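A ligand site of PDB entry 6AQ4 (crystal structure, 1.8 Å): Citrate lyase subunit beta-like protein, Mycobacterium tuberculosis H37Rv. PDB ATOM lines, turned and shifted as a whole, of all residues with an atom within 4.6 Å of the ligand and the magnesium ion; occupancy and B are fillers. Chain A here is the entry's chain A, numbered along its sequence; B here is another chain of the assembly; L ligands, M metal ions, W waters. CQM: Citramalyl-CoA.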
ATOM      1  N   LEU A  19     -15.953 -31.518  -3.162  1.00  0.00           N
ATOM      2  CA  LEU A  19     -15.756 -30.216  -3.787  1.00  0.00           C
ATOM      3  C   LEU A  19     -16.938 -29.262  -3.541  1.00  0.00           C
ATOM      4  O   LEU A  19     -18.073 -29.561  -3.876  1.00  0.00           O
ATOM      5  CB  LEU A  19     -15.529 -30.393  -5.293  1.00  0.00           C
ATOM      6  CG  LEU A  19     -15.486 -29.134  -6.152  1.00  0.00           C
ATOM      7  CD1 LEU A  19     -14.250 -28.263  -5.808  1.00  0.00           C
ATOM      8  CD2 LEU A  19     -15.466 -29.522  -7.621  1.00  0.00           C
ATOM      9  N   PHE A  20     -16.639 -28.092  -2.953  1.00  0.00           N
ATOM     10  CA  PHE A  20     -17.608 -27.005  -2.843  1.00  0.00           C
ATOM     11  C   PHE A  20     -17.893 -26.413  -4.211  1.00  0.00           C
ATOM     12  O   PHE A  20     -16.972 -26.231  -5.025  1.00  0.00           O
ATOM     13  CB  PHE A  20     -17.082 -25.881  -1.959  1.00  0.00           C
ATOM     14  CG  PHE A  20     -17.389 -26.017  -0.492  1.00  0.00           C
ATOM     15  CD1 PHE A  20     -18.687 -25.891  -0.018  1.00  0.00           C
ATOM     16  CD2 PHE A  20     -16.350 -26.206   0.426  1.00  0.00           C
ATOM     17  CE1 PHE A  20     -18.955 -25.997   1.333  1.00  0.00           C
ATOM     18  CE2 PHE A  20     -16.620 -26.317   1.769  1.00  0.00           C
ATOM     19  CZ  PHE A  20     -17.923 -26.203   2.228  1.00  0.00           C
ATOM     20  N   CYS A  21     -19.143 -26.085  -4.472  1.00  0.00           N
ATOM     21  CA  CYS A  21     -19.501 -25.317  -5.653  1.00  0.00           C
ATOM     22  C   CYS A  21     -20.676 -24.409  -5.306  1.00  0.00           C
ATOM     23  O   CYS A  21     -21.741 -24.902  -4.950  1.00  0.00           O
ATOM     24  CB  CYS A  21     -19.888 -26.232  -6.803  1.00  0.00           C
ATOM     25  SG  CYS A  21     -20.327 -25.325  -8.309  1.00  0.00           S
ATOM     26  N   PRO A  22     -20.490 -23.085  -5.402  1.00  0.00           N
ATOM     27  CA  PRO A  22     -21.601 -22.173  -5.106  1.00  0.00           C
ATOM     28  C   PRO A  22     -22.815 -22.520  -5.972  1.00  0.00           C
ATOM     29  O   PRO A  22     -22.666 -22.721  -7.183  1.00  0.00           O
ATOM     30  CB  PRO A  22     -21.041 -20.787  -5.478  1.00  0.00           C
ATOM     31  CG  PRO A  22     -19.549 -20.953  -5.505  1.00  0.00           C
ATOM     32  CD  PRO A  22     -19.311 -22.383  -5.924  1.00  0.00           C
ATOM     33  N   ARG A  28     -21.812 -24.815 -13.650  1.00  0.00           N
ATOM     34  CA  ARG A  28     -20.625 -25.510 -13.139  1.00  0.00           C
ATOM     35  C   ARG A  28     -20.917 -26.858 -12.473  1.00  0.00           C
ATOM     36  O   ARG A  28     -20.001 -27.648 -12.235  1.00  0.00           O
ATOM     37  CB  ARG A  28     -19.841 -24.617 -12.178  1.00  0.00           C
ATOM     38  CG  ARG A  28     -19.166 -23.455 -12.896  1.00  0.00           C
ATOM     39  CD  ARG A  28     -18.283 -22.641 -11.982  1.00  0.00           C
ATOM     40  NE  ARG A  28     -17.633 -21.553 -12.725  1.00  0.00           N
ATOM     41  CZ  ARG A  28     -16.616 -20.837 -12.252  1.00  0.00           C
ATOM     42  NH1 ARG A  28     -16.127 -21.104 -11.054  1.00  0.00           N
ATOM     43  NH2 ARG A  28     -16.075 -19.879 -12.988  1.00  0.00           N
ATOM     44  N   LYS A  31     -19.604 -30.173 -14.126  1.00  0.00           N
ATOM     45  CA  LYS A  31     -18.159 -30.292 -14.083  1.00  0.00           C
ATOM     46  C   LYS A  31     -17.695 -30.657 -12.666  1.00  0.00           C
ATOM     47  O   LYS A  31     -16.799 -31.476 -12.477  1.00  0.00           O
ATOM     48  CB  LYS A  31     -17.486 -28.996 -14.564  1.00  0.00           C
ATOM     49  CG  LYS A  31     -17.860 -28.601 -15.996  1.00  0.00           C
ATOM     50  CD  LYS A  31     -17.119 -27.350 -16.476  1.00  0.00           C
ATOM     51  CE  LYS A  31     -17.621 -26.081 -15.763  1.00  0.00           C
ATOM     52  NZ  LYS A  31     -17.020 -24.832 -16.329  1.00  0.00           N
ATOM     53  N   ALA A  32     -18.332 -30.056 -11.661  1.00  0.00           N
ATOM     54  CA  ALA A  32     -17.984 -30.383 -10.290  1.00  0.00           C
ATOM     55  C   ALA A  32     -18.272 -31.854  -9.989  1.00  0.00           C
ATOM     56  O   ALA A  32     -17.446 -32.535  -9.373  1.00  0.00           O
ATOM     57  CB  ALA A  32     -18.705 -29.480  -9.317  1.00  0.00           C
ATOM     58  N   ASP A  42     -23.322 -25.099  -2.507  1.00  0.00           N
ATOM     59  CA  ASP A  42     -23.308 -24.134  -1.410  1.00  0.00           C
ATOM     60  C   ASP A  42     -24.377 -23.057  -1.525  1.00  0.00           C
ATOM     61  O   ASP A  42     -24.475 -22.371  -2.538  1.00  0.00           O
ATOM     62  CB  ASP A  42     -21.924 -23.479  -1.297  1.00  0.00           C
ATOM     63  CG  ASP A  42     -21.758 -22.652  -0.018  1.00  0.00           C
ATOM     64  OD1 ASP A  42     -22.494 -22.897   0.973  1.00  0.00           O
ATOM     65  OD2 ASP A  42     -20.880 -21.770  -0.005  1.00  0.00           O
ATOM     66  N   GLU A  44     -24.633 -21.077   1.356  1.00  0.00           N
ATOM     67  CA  GLU A  44     -24.152 -20.148   2.387  1.00  0.00           C
ATOM     68  C   GLU A  44     -23.078 -19.171   1.861  1.00  0.00           C
ATOM     69  O   GLU A  44     -23.306 -18.438   0.905  1.00  0.00           O
ATOM     70  CB  GLU A  44     -23.670 -20.913   3.631  1.00  0.00           C
ATOM     71  CG  GLU A  44     -23.744 -20.095   4.915  1.00  0.00           C
ATOM     72  CD  GLU A  44     -22.475 -20.179   5.768  1.00  0.00           C
ATOM     73  OE1 GLU A  44     -21.395 -20.483   5.216  1.00  0.00           O
ATOM     74  OE2 GLU A  44     -22.558 -19.960   6.996  1.00  0.00           O
ATOM     75  N   ASP A  45     -21.893 -19.173   2.489  1.00  0.00           N
ATOM     76  CA  ASP A  45     -20.885 -18.113   2.263  1.00  0.00           C
ATOM     77  C   ASP A  45     -20.274 -17.993   0.857  1.00  0.00           C
ATOM     78  O   ASP A  45     -19.697 -16.956   0.523  1.00  0.00           O
ATOM     79  CB  ASP A  45     -19.754 -18.177   3.303  1.00  0.00           C
ATOM     80  CG  ASP A  45     -20.165 -17.608   4.632  1.00  0.00           C
ATOM     81  OD1 ASP A  45     -21.247 -16.983   4.700  1.00  0.00           O
ATOM     82  OD2 ASP A  45     -19.411 -17.769   5.605  1.00  0.00           O
ATOM     83  N   GLY A  46     -20.384 -19.034   0.037  1.00  0.00           N
ATOM     84  CA  GLY A  46     -19.909 -18.976  -1.328  1.00  0.00           C
ATOM     85  C   GLY A  46     -20.833 -18.152  -2.214  1.00  0.00           C
ATOM     86  O   GLY A  46     -20.495 -17.846  -3.351  1.00  0.00           O
ATOM     87  N   ARG A  72     -24.925 -27.362   1.412  1.00  0.00           N
ATOM     88  CA  ARG A  72     -24.684 -26.510   2.568  1.00  0.00           C
ATOM     89  C   ARG A  72     -25.744 -25.422   2.653  1.00  0.00           C
ATOM     90  O   ARG A  72     -25.811 -24.529   1.794  1.00  0.00           O
ATOM     91  CB  ARG A  72     -23.284 -25.905   2.597  1.00  0.00           C
ATOM     92  CG  ARG A  72     -23.067 -25.054   3.853  1.00  0.00           C
ATOM     93  CD  ARG A  72     -21.608 -24.717   4.054  1.00  0.00           C
ATOM     94  NE  ARG A  72     -21.150 -23.659   3.145  1.00  0.00           N
ATOM     95  CZ  ARG A  72     -20.033 -22.969   3.328  1.00  0.00           C
ATOM     96  NH1 ARG A  72     -19.268 -23.232   4.394  1.00  0.00           N
ATOM     97  NH2 ARG A  72     -19.681 -22.019   2.461  1.00  0.00           N
ATOM     98  N   LYS A 100     -21.623 -22.958  11.011  1.00  0.00           N
ATOM     99  CA  LYS A 100     -21.738 -22.395  12.356  1.00  0.00           C
ATOM    100  C   LYS A 100     -22.549 -23.327  13.290  1.00  0.00           C
ATOM    101  O   LYS A 100     -23.371 -22.873  14.088  1.00  0.00           O
ATOM    102  CB  LYS A 100     -22.369 -20.986  12.309  1.00  0.00           C
ATOM    103  CG  LYS A 100     -21.446 -19.877  11.779  1.00  0.00           C
ATOM    104  CD  LYS A 100     -21.602 -19.667  10.268  1.00  0.00           C
ATOM    105  CE  LYS A 100     -20.659 -18.548   9.776  1.00  0.00           C
ATOM    106  NZ  LYS A 100     -20.687 -18.320   8.303  1.00  0.00           N
ATOM    107  N   LEU A 118     -20.693 -28.444  10.374  1.00  0.00           N
ATOM    108  CA  LEU A 118     -19.470 -27.684  10.136  1.00  0.00           C
ATOM    109  C   LEU A 118     -19.203 -26.782  11.322  1.00  0.00           C
ATOM    110  O   LEU A 118     -19.874 -25.756  11.517  1.00  0.00           O
ATOM    111  CB  LEU A 118     -19.568 -26.909   8.799  1.00  0.00           C
ATOM    112  CG  LEU A 118     -18.541 -25.805   8.532  1.00  0.00           C
ATOM    113  CD1 LEU A 118     -17.110 -26.356   8.530  1.00  0.00           C
ATOM    114  CD2 LEU A 118     -18.838 -25.077   7.204  1.00  0.00           C
ATOM    115  N   GLU A 120     -17.129 -24.151  13.313  1.00  0.00           N
ATOM    116  CA  GLU A 120     -16.305 -23.060  12.830  1.00  0.00           C
ATOM    117  C   GLU A 120     -16.489 -21.797  13.671  1.00  0.00           C
ATOM    118  O   GLU A 120     -16.337 -20.663  13.170  1.00  0.00           O
ATOM    119  CB  GLU A 120     -16.642 -22.772  11.354  1.00  0.00           C
ATOM    120  CG  GLU A 120     -18.114 -22.469  11.119  1.00  0.00           C
ATOM    121  CD  GLU A 120     -18.397 -22.227   9.663  1.00  0.00           C
ATOM    122  OE1 GLU A 120     -17.415 -22.012   8.948  1.00  0.00           O
ATOM    123  OE2 GLU A 120     -19.564 -22.277   9.230  1.00  0.00           O
ATOM    124  N   MET A 141     -17.160 -31.405  10.173  1.00  0.00           N
ATOM    125  CA  MET A 141     -16.129 -30.665   9.455  1.00  0.00           C
ATOM    126  C   MET A 141     -15.761 -29.475  10.324  1.00  0.00           C
ATOM    127  O   MET A 141     -16.555 -29.055  11.167  1.00  0.00           O
ATOM    128  CB  MET A 141     -16.655 -30.182   8.109  1.00  0.00           C
ATOM    129  CG  MET A 141     -15.651 -29.405   7.251  1.00  0.00           C
ATOM    130  SD  MET A 141     -16.380 -28.995   5.657  1.00  0.00           S
ATOM    131  CE  MET A 141     -15.023 -28.043   4.915  1.00  0.00           C
ATOM    132  N   GLY A 143     -13.964 -25.378  10.174  1.00  0.00           N
ATOM    133  CA  GLY A 143     -13.788 -24.249   9.272  1.00  0.00           C
ATOM    134  C   GLY A 143     -12.873 -23.239   9.937  1.00  0.00           C
ATOM    135  O   GLY A 143     -13.261 -22.598  10.909  1.00  0.00           O
ATOM    136  N   ALA A 144     -11.663 -23.094   9.406  1.00  0.00           N
ATOM    137  CA  ALA A 144     -10.625 -22.300  10.060  1.00  0.00           C
ATOM    138  C   ALA A 144     -10.957 -20.827   9.958  1.00  0.00           C
ATOM    139  O   ALA A 144     -10.636 -20.047  10.840  1.00  0.00           O
ATOM    140  CB  ALA A 144      -9.257 -22.574   9.431  1.00  0.00           C
ATOM    141  N   GLU A 145     -11.616 -20.441   8.876  1.00  0.00           N
ATOM    142  CA  GLU A 145     -11.747 -19.021   8.567  1.00  0.00           C
ATOM    143  C   GLU A 145     -12.846 -18.335   9.360  1.00  0.00           C
ATOM    144  O   GLU A 145     -12.607 -17.284   9.958  1.00  0.00           O
ATOM    145  CB  GLU A 145     -11.906 -18.798   7.060  1.00  0.00           C
ATOM    146  CG  GLU A 145     -10.804 -19.494   6.248  1.00  0.00           C
ATOM    147  CD  GLU A 145      -9.380 -19.053   6.653  1.00  0.00           C
ATOM    148  OE1 GLU A 145      -9.158 -17.853   6.937  1.00  0.00           O
ATOM    149  OE2 GLU A 145      -8.481 -19.921   6.680  1.00  0.00           O
ATOM    150  N   ASP A 146     -14.047 -18.915   9.406  1.00  0.00           N
ATOM    151  CA  ASP A 146     -15.050 -18.397  10.330  1.00  0.00           C
ATOM    152  C   ASP A 146     -14.617 -18.540  11.790  1.00  0.00           C
ATOM    153  O   ASP A 146     -14.951 -17.701  12.611  1.00  0.00           O
ATOM    154  CB  ASP A 146     -16.443 -19.011  10.108  1.00  0.00           C
ATOM    155  CG  ASP A 146     -17.294 -18.165   9.194  1.00  0.00           C
ATOM    156  OD1 ASP A 146     -17.372 -16.939   9.408  1.00  0.00           O
ATOM    157  OD2 ASP A 146     -17.870 -18.709   8.242  1.00  0.00           O
ATOM    158  N   VAL A 189     -10.751 -26.848   3.995  1.00  0.00           N
ATOM    159  CA  VAL A 189     -10.351 -26.467   2.645  1.00  0.00           C
ATOM    160  C   VAL A 189      -8.970 -25.823   2.648  1.00  0.00           C
ATOM    161  O   VAL A 189      -8.524 -25.256   3.663  1.00  0.00           O
ATOM    162  CB  VAL A 189     -11.394 -25.527   1.995  1.00  0.00           C
ATOM    163  CG1 VAL A 189     -12.772 -26.213   1.893  1.00  0.00           C
ATOM    164  CG2 VAL A 189     -11.493 -24.224   2.777  1.00  0.00           C
ATOM    165  N   ILE A 193      -5.155 -21.977  -4.030  1.00  0.00           N
ATOM    166  CA  ILE A 193      -5.560 -22.951  -5.047  1.00  0.00           C
ATOM    167  C   ILE A 193      -4.381 -23.620  -5.720  1.00  0.00           C
ATOM    168  O   ILE A 193      -4.366 -24.845  -5.876  1.00  0.00           O
ATOM    169  CB  ILE A 193      -6.467 -22.316  -6.117  1.00  0.00           C
ATOM    170  CG1 ILE A 193      -7.742 -21.759  -5.468  1.00  0.00           C
ATOM    171  CG2 ILE A 193      -6.800 -23.328  -7.220  1.00  0.00           C
ATOM    172  CD1 ILE A 193      -8.495 -20.775  -6.339  1.00  0.00           C
ATOM    173  N   ILE A 217     -11.883 -26.573  -2.806  1.00  0.00           N
ATOM    174  CA  ILE A 217     -12.595 -25.409  -3.345  1.00  0.00           C
ATOM    175  C   ILE A 217     -12.331 -25.195  -4.835  1.00  0.00           C
ATOM    176  O   ILE A 217     -12.782 -24.209  -5.421  1.00  0.00           O
ATOM    177  CB  ILE A 217     -12.291 -24.108  -2.533  1.00  0.00           C
ATOM    178  CG1 ILE A 217     -10.809 -23.991  -2.150  1.00  0.00           C
ATOM    179  CG2 ILE A 217     -13.148 -24.062  -1.262  1.00  0.00           C
ATOM    180  CD1 ILE A 217      -9.870 -23.709  -3.289  1.00  0.00           C
ATOM    181  N   HIS A 218     -11.614 -26.134  -5.460  1.00  0.00           N
ATOM    182  CA  HIS A 218     -11.329 -26.048  -6.893  1.00  0.00           C
ATOM    183  C   HIS A 218     -11.091 -27.455  -7.437  1.00  0.00           C
ATOM    184  O   HIS A 218     -10.416 -28.263  -6.802  1.00  0.00           O
ATOM    185  CB  HIS A 218     -10.099 -25.156  -7.122  1.00  0.00           C
ATOM    186  CG  HIS A 218      -9.895 -24.746  -8.551  1.00  0.00           C
ATOM    187  ND1 HIS A 218      -9.586 -25.651  -9.550  1.00  0.00           N
ATOM    188  CD2 HIS A 218      -9.972 -23.538  -9.157  1.00  0.00           C
ATOM    189  CE1 HIS A 218      -9.477 -25.012 -10.696  1.00  0.00           C
ATOM    190  NE2 HIS A 218      -9.703 -23.735 -10.489  1.00  0.00           N
ATOM    191  N   PRO A 219     -11.652 -27.766  -8.621  1.00  0.00           N
ATOM    192  CA  PRO A 219     -11.518 -29.079  -9.274  1.00  0.00           C
ATOM    193  C   PRO A 219     -10.055 -29.561  -9.341  1.00  0.00           C
ATOM    194  O   PRO A 219      -9.811 -30.759  -9.194  1.00  0.00           O
ATOM    195  CB  PRO A 219     -12.015 -28.815 -10.705  1.00  0.00           C
ATOM    196  CG  PRO A 219     -12.930 -27.677 -10.575  1.00  0.00           C
ATOM    197  CD  PRO A 219     -12.407 -26.820  -9.461  1.00  0.00           C
ATOM    198  N   ALA B 252     -17.924 -16.132  -3.455  1.00  0.00           N
ATOM    199  CA  ALA B 252     -16.536 -16.555  -3.586  1.00  0.00           C
ATOM    200  C   ALA B 252     -15.857 -16.020  -4.832  1.00  0.00           C
ATOM    201  O   ALA B 252     -16.472 -15.939  -5.907  1.00  0.00           O
ATOM    202  CB  ALA B 252     -16.448 -18.080  -3.549  1.00  0.00           C
ATOM    203  N   PHE B 253     -14.579 -15.657  -4.688  1.00  0.00           N
ATOM    204  CA  PHE B 253     -13.769 -15.288  -5.843  1.00  0.00           C
ATOM    205  C   PHE B 253     -12.305 -15.522  -5.502  1.00  0.00           C
ATOM    206  O   PHE B 253     -11.938 -15.632  -4.326  1.00  0.00           O
ATOM    207  CB  PHE B 253     -14.019 -13.824  -6.256  1.00  0.00           C
ATOM    208  CG  PHE B 253     -13.485 -12.814  -5.270  1.00  0.00           C
ATOM    209  CD1 PHE B 253     -12.292 -12.152  -5.498  1.00  0.00           C
ATOM    210  CD2 PHE B 253     -14.201 -12.514  -4.116  1.00  0.00           C
ATOM    211  CE1 PHE B 253     -11.798 -11.229  -4.588  1.00  0.00           C
ATOM    212  CE2 PHE B 253     -13.723 -11.596  -3.196  1.00  0.00           C
ATOM    213  CZ  PHE B 253     -12.519 -10.945  -3.432  1.00  0.00           C
ATOM    214  N   ALA B 254     -11.472 -15.597  -6.531  1.00  0.00           N
ATOM    215  CA  ALA B 254     -10.042 -15.817  -6.335  1.00  0.00           C
ATOM    216  C   ALA B 254      -9.306 -14.498  -6.285  1.00  0.00           C
ATOM    217  O   ALA B 254      -9.441 -13.668  -7.191  1.00  0.00           O
ATOM    218  CB  ALA B 254      -9.482 -16.707  -7.439  1.00  0.00           C
ATOM    219  N   MET B 259      -8.756 -18.436  -2.539  1.00  0.00           N
ATOM    220  CA  MET B 259     -10.201 -18.350  -2.542  1.00  0.00           C
ATOM    221  C   MET B 259     -10.631 -17.374  -1.456  1.00  0.00           C
ATOM    222  O   MET B 259     -10.234 -17.501  -0.302  1.00  0.00           O
ATOM    223  CB  MET B 259     -10.828 -19.733  -2.297  1.00  0.00           C
ATOM    224  CG  MET B 259     -12.280 -19.844  -2.708  1.00  0.00           C
ATOM    225  SD  MET B 259     -13.401 -19.229  -1.440  1.00  0.00           S
ATOM    226  CE  MET B 259     -12.981 -20.303  -0.084  1.00  0.00           C
ATOM    227  N   ASP B 261     -13.955 -15.414   0.401  1.00  0.00           N
ATOM    228  CA  ASP B 261     -15.369 -15.145   0.677  1.00  0.00           C
ATOM    229  C   ASP B 261     -15.546 -14.561   2.091  1.00  0.00           C
ATOM    230  O   ASP B 261     -14.579 -14.204   2.764  1.00  0.00           O
ATOM    231  CB  ASP B 261     -16.261 -16.387   0.483  1.00  0.00           C
ATOM    232  CG  ASP B 261     -15.928 -17.516   1.447  1.00  0.00           C
ATOM    233  OD1 ASP B 261     -15.223 -17.280   2.461  1.00  0.00           O
ATOM    234  OD2 ASP B 261     -16.374 -18.654   1.198  1.00  0.00           O
ATOM    235  N   PRO B 263     -15.813 -14.747   5.494  1.00  0.00           N
ATOM    236  CA  PRO B 263     -14.988 -14.595   6.709  1.00  0.00           C
ATOM    237  C   PRO B 263     -13.592 -14.005   6.406  1.00  0.00           C
ATOM    238  O   PRO B 263     -12.997 -13.336   7.266  1.00  0.00           O
ATOM    239  CB  PRO B 263     -14.864 -16.032   7.234  1.00  0.00           C
ATOM    240  CG  PRO B 263     -15.015 -16.890   6.001  1.00  0.00           C
ATOM    241  CD  PRO B 263     -16.013 -16.162   5.137  1.00  0.00           C
HETATM  242  C2  CQM L   1     -14.746 -21.564   4.337  1.00  0.00           C
HETATM  243  C4  CQM L   1     -14.484 -21.561   6.701  1.00  0.00           C
HETATM  244  C6  CQM L   1     -14.908 -23.750   5.399  1.00  0.00           C
HETATM  245  P2A CQM L   1     -12.587 -19.170 -11.276  1.00  0.00           P
HETATM  246  O5A CQM L   1     -13.592 -19.232 -12.387  1.00  0.00           O
HETATM  247  O4A CQM L   1     -11.889 -17.822 -11.172  1.00  0.00           O
HETATM  248  O3A CQM L   1     -11.510 -20.304 -11.342  1.00  0.00           O
HETATM  249  O6A CQM L   1     -13.366 -19.417  -9.899  1.00  0.00           O
HETATM  250  P1A CQM L   1     -10.890 -20.971 -12.632  1.00  0.00           P
HETATM  251  O1A CQM L   1      -9.528 -21.513 -12.222  1.00  0.00           O
HETATM  252  O2A CQM L   1     -10.755 -19.970 -13.776  1.00  0.00           O
HETATM  253  O5B CQM L   1     -11.796 -22.185 -13.070  1.00  0.00           O
HETATM  254  C5B CQM L   1     -11.431 -22.993 -14.138  1.00  0.00           C
HETATM  255  C4B CQM L   1     -12.481 -24.001 -14.603  1.00  0.00           C
HETATM  256  O4B CQM L   1     -12.829 -24.772 -13.524  1.00  0.00           O
HETATM  257  C3B CQM L   1     -13.727 -23.346 -15.036  1.00  0.00           C
HETATM  258  O3B CQM L   1     -14.377 -24.141 -16.000  1.00  0.00           O
HETATM  259  C2B CQM L   1     -14.517 -23.254 -13.889  1.00  0.00           C
HETATM  260  O2B CQM L   1     -15.857 -23.128 -14.196  1.00  0.00           O
HETATM  261  C1B CQM L   1     -14.067 -24.385 -13.054  1.00  0.00           C
HETATM  262  P3B CQM L   1     -13.944 -24.088 -17.534  1.00  0.00           P
HETATM  263  O7A CQM L   1     -15.114 -24.604 -18.371  1.00  0.00           O
HETATM  264  O8A CQM L   1     -12.715 -24.969 -17.760  1.00  0.00           O
HETATM  265  O9A CQM L   1     -13.590 -22.666 -17.935  1.00  0.00           O
HETATM  266  N9A CQM L   1     -14.262 -24.308 -11.596  1.00  0.00           N
HETATM  267  C4A CQM L   1     -15.221 -24.958 -10.908  1.00  0.00           C
HETATM  268  N3A CQM L   1     -16.209 -25.788 -11.285  1.00  0.00           N
HETATM  269  C2A CQM L   1     -17.026 -26.295 -10.362  1.00  0.00           C
HETATM  270  N1A CQM L   1     -16.893 -25.996  -9.056  1.00  0.00           N
HETATM  271  C6A CQM L   1     -15.919 -25.174  -8.628  1.00  0.00           C
HETATM  272  C5A CQM L   1     -15.046 -24.631  -9.559  1.00  0.00           C
HETATM  273  N7A CQM L   1     -13.999 -23.789  -9.476  1.00  0.00           N
HETATM  274  C8A CQM L   1     -13.513 -23.602 -10.725  1.00  0.00           C
HETATM  275  N6A CQM L   1     -15.779 -24.878  -7.216  1.00  0.00           N
HETATM  276  CBP CQM L   1     -13.587 -19.650  -7.519  1.00  0.00           C
HETATM  277  CCP CQM L   1     -12.703 -19.353  -8.679  1.00  0.00           C
HETATM  278  CDP CQM L   1     -14.726 -18.691  -7.557  1.00  0.00           C
HETATM  279  CEP CQM L   1     -12.813 -19.494  -6.185  1.00  0.00           C
HETATM  280  CAP CQM L   1     -14.103 -21.065  -7.708  1.00  0.00           C
HETATM  281  OAP CQM L   1     -13.053 -22.002  -7.660  1.00  0.00           O
HETATM  282  C9P CQM L   1     -15.072 -21.456  -6.603  1.00  0.00           C
HETATM  283  O9P CQM L   1     -16.179 -20.972  -6.559  1.00  0.00           O
HETATM  284  N8P CQM L   1     -14.647 -22.397  -5.596  1.00  0.00           N
HETATM  285  C7P CQM L   1     -15.517 -22.775  -4.521  1.00  0.00           C
HETATM  286  C6P CQM L   1     -16.109 -21.597  -3.732  1.00  0.00           C
HETATM  287  C5P CQM L   1     -16.915 -21.986  -2.522  1.00  0.00           C
HETATM  288  O5P CQM L   1     -17.853 -22.757  -2.645  1.00  0.00           O
HETATM  289  N4P CQM L   1     -16.574 -21.426  -1.243  1.00  0.00           N
HETATM  290  C3P CQM L   1     -17.342 -21.807  -0.066  1.00  0.00           C
HETATM  291  C2P CQM L   1     -16.612 -22.835   0.782  1.00  0.00           C
HETATM  292  S1P CQM L   1     -15.094 -22.240   1.550  1.00  0.00           S
HETATM  293  C1  CQM L   1     -15.657 -21.496   3.117  1.00  0.00           C
HETATM  294  O2  CQM L   1     -16.777 -20.927   3.230  1.00  0.00           O
HETATM  295  C3  CQM L   1     -15.241 -22.266   5.580  1.00  0.00           C
HETATM  296  O7  CQM L   1     -16.593 -22.123   5.819  1.00  0.00           O
HETATM  297  O3  CQM L   1     -15.074 -20.728   7.504  1.00  0.00           O
HETATM  298  O4  CQM L   1     -13.256 -21.792   6.825  1.00  0.00           O
HETATM  299 MG    MG M   1     -17.483 -20.620   7.197  1.00  0.00          MG
HETATM  300  O   HOH W   1     -11.425 -23.436   6.451  1.00  0.00           O
HETATM  301  O   HOH W   2     -16.309 -21.294 -16.235  1.00  0.00           O
HETATM  302  O   HOH W   3     -13.084 -19.824 -15.478  1.00  0.00           O
HETATM  303  O   HOH W   4     -12.452 -15.832  -9.312  1.00  0.00           O
HETATM  304  O   HOH W   5     -17.657 -19.232   5.336  1.00  0.00           O
HETATM  305  O   HOH W   6     -19.577 -21.033   6.865  1.00  0.00           O
HETATM  306  O   HOH W   7     -12.874 -25.726   6.024  1.00  0.00           O
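The backbone NH (N) of Asp 146 lies close to an oxygen (O3) of the ligand. The backbone carbonyl oxygen of Ile 217 lies within hydrogen-bond range of a nitrogen (N8P) of the ligand, at 2.6 Å. NH2 of Arg 28 lies within salt-bridge range of O5A of the ligand (2.6 Å). The side-chain amino group (NZ) of Lys 31 lies within salt-bridge range of an oxygen (O7A) of the ligand. An oxygen (O1A) of the ligand is in hydrogen-bond range of a ring nitrogen (NE2) of His 218 (2.8 Å). The backbone carbonyl oxygen of Phe 20 is in hydrogen-bond range of a nitrogen (N6A) of the ligand (2.8 Å). O4 of the ligand lies within hydrogen-bond range of N of Glu 145, at 3.0 Å. O2 of the ligand sits at hydrogen-bond distance from NH2 of Arg 72 (3.2 Å). N of Ala 144 is in hydrogen-bond range of O4 of the ligand (3.3 Å). A nitrogen (N1A) of the ligand is in hydrogen-bond range of the side-chain sulfur of Cys 21.
NZ of Lys 100 is in salt-bridge range of OD1 of Asp 146, at 3.8 Å. OE2 of Glu 120 lies within hydrogen-bond range of N of Lys 100 (2.8 Å). OD1 of Asp 42 is in salt-bridge range of NE of Arg 72 (2.7 Å). NH1 of Arg 72 is in salt-bridge range of OE1 of Glu 44. N of Ala 252 of chain B lies within hydrogen-bond range of O of Gly 46 (3.1 Å). OD2 of Asp 42 sits at hydrogen-bond distance from N of Gly 46 (2.8 Å). The side-chain carboxylate (OD1) of Asp 42 lies within hydrogen-bond range of the backbone NH (N) of Glu 44 (2.8 Å). N of Lys 100 sits at hydrogen-bond distance from O of Leu 118 (3.3 Å).
OD2 of Asp 261 of chain B sits close to O2 of the ligand (3.1 Å). Residues that only touch the ligand: Leu 19, Pro 22, Ala 32, Asp 42, Leu 118, Gly 143, Pro 219, Ala 252 of chain B, Phe 253 of chain B and Met 259 of chain B. 22 residues have an atom within 4 Å of the ligand: Leu 19, Phe 20, Cys 21, Pro 22, Arg 28, Lys 31, Ala 32, Asp 42, Arg 72, Leu 118, Glu 120, Gly 143, Ala 144, Glu 145, Asp 146, Ile 217, His 218, Pro 219, Ala 252 of chain B, Phe 253 of chain B, Met 259 of chain B and Asp 261 of chain B. The nearest printed residue that does not touch the ligand is Gly 46 (4.02 Å).
OD2 of Asp 45 touches the magnesium ion, 3.8 Å away. Of the 31 residues printed, 3 come within 4 Å of the magnesium ion. The nearest printed residue that does not touch the magnesium ion is Lys 100 (4.1 Å).
The magnesium ion is bound by water W6 (2.2 Å), OD2 of Asp 146 (2.2 Å), O7 of the ligand (2.2 Å), OE1 of Glu 120 (2.2 Å), water W5 (2.3 Å) and O3 of the ligand (2.4 Å). The magnesium ion has six donor atoms within binding distance.
Water W6 lies within hydrogen-bond range of OE1 of Glu 44, OE2 of Glu 120, NZ of Lys 100 and NH1 of Arg 72. Water W1 lies within hydrogen-bond range of an oxygen (O4) of the ligand (2.5 Å) and the backbone NH (N) of Ala 144 (3.0 Å). Water W4 lies within hydrogen-bond range of O4A of the ligand (2.8 Å) and N of Ala 254 of chain B (3.0 Å).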
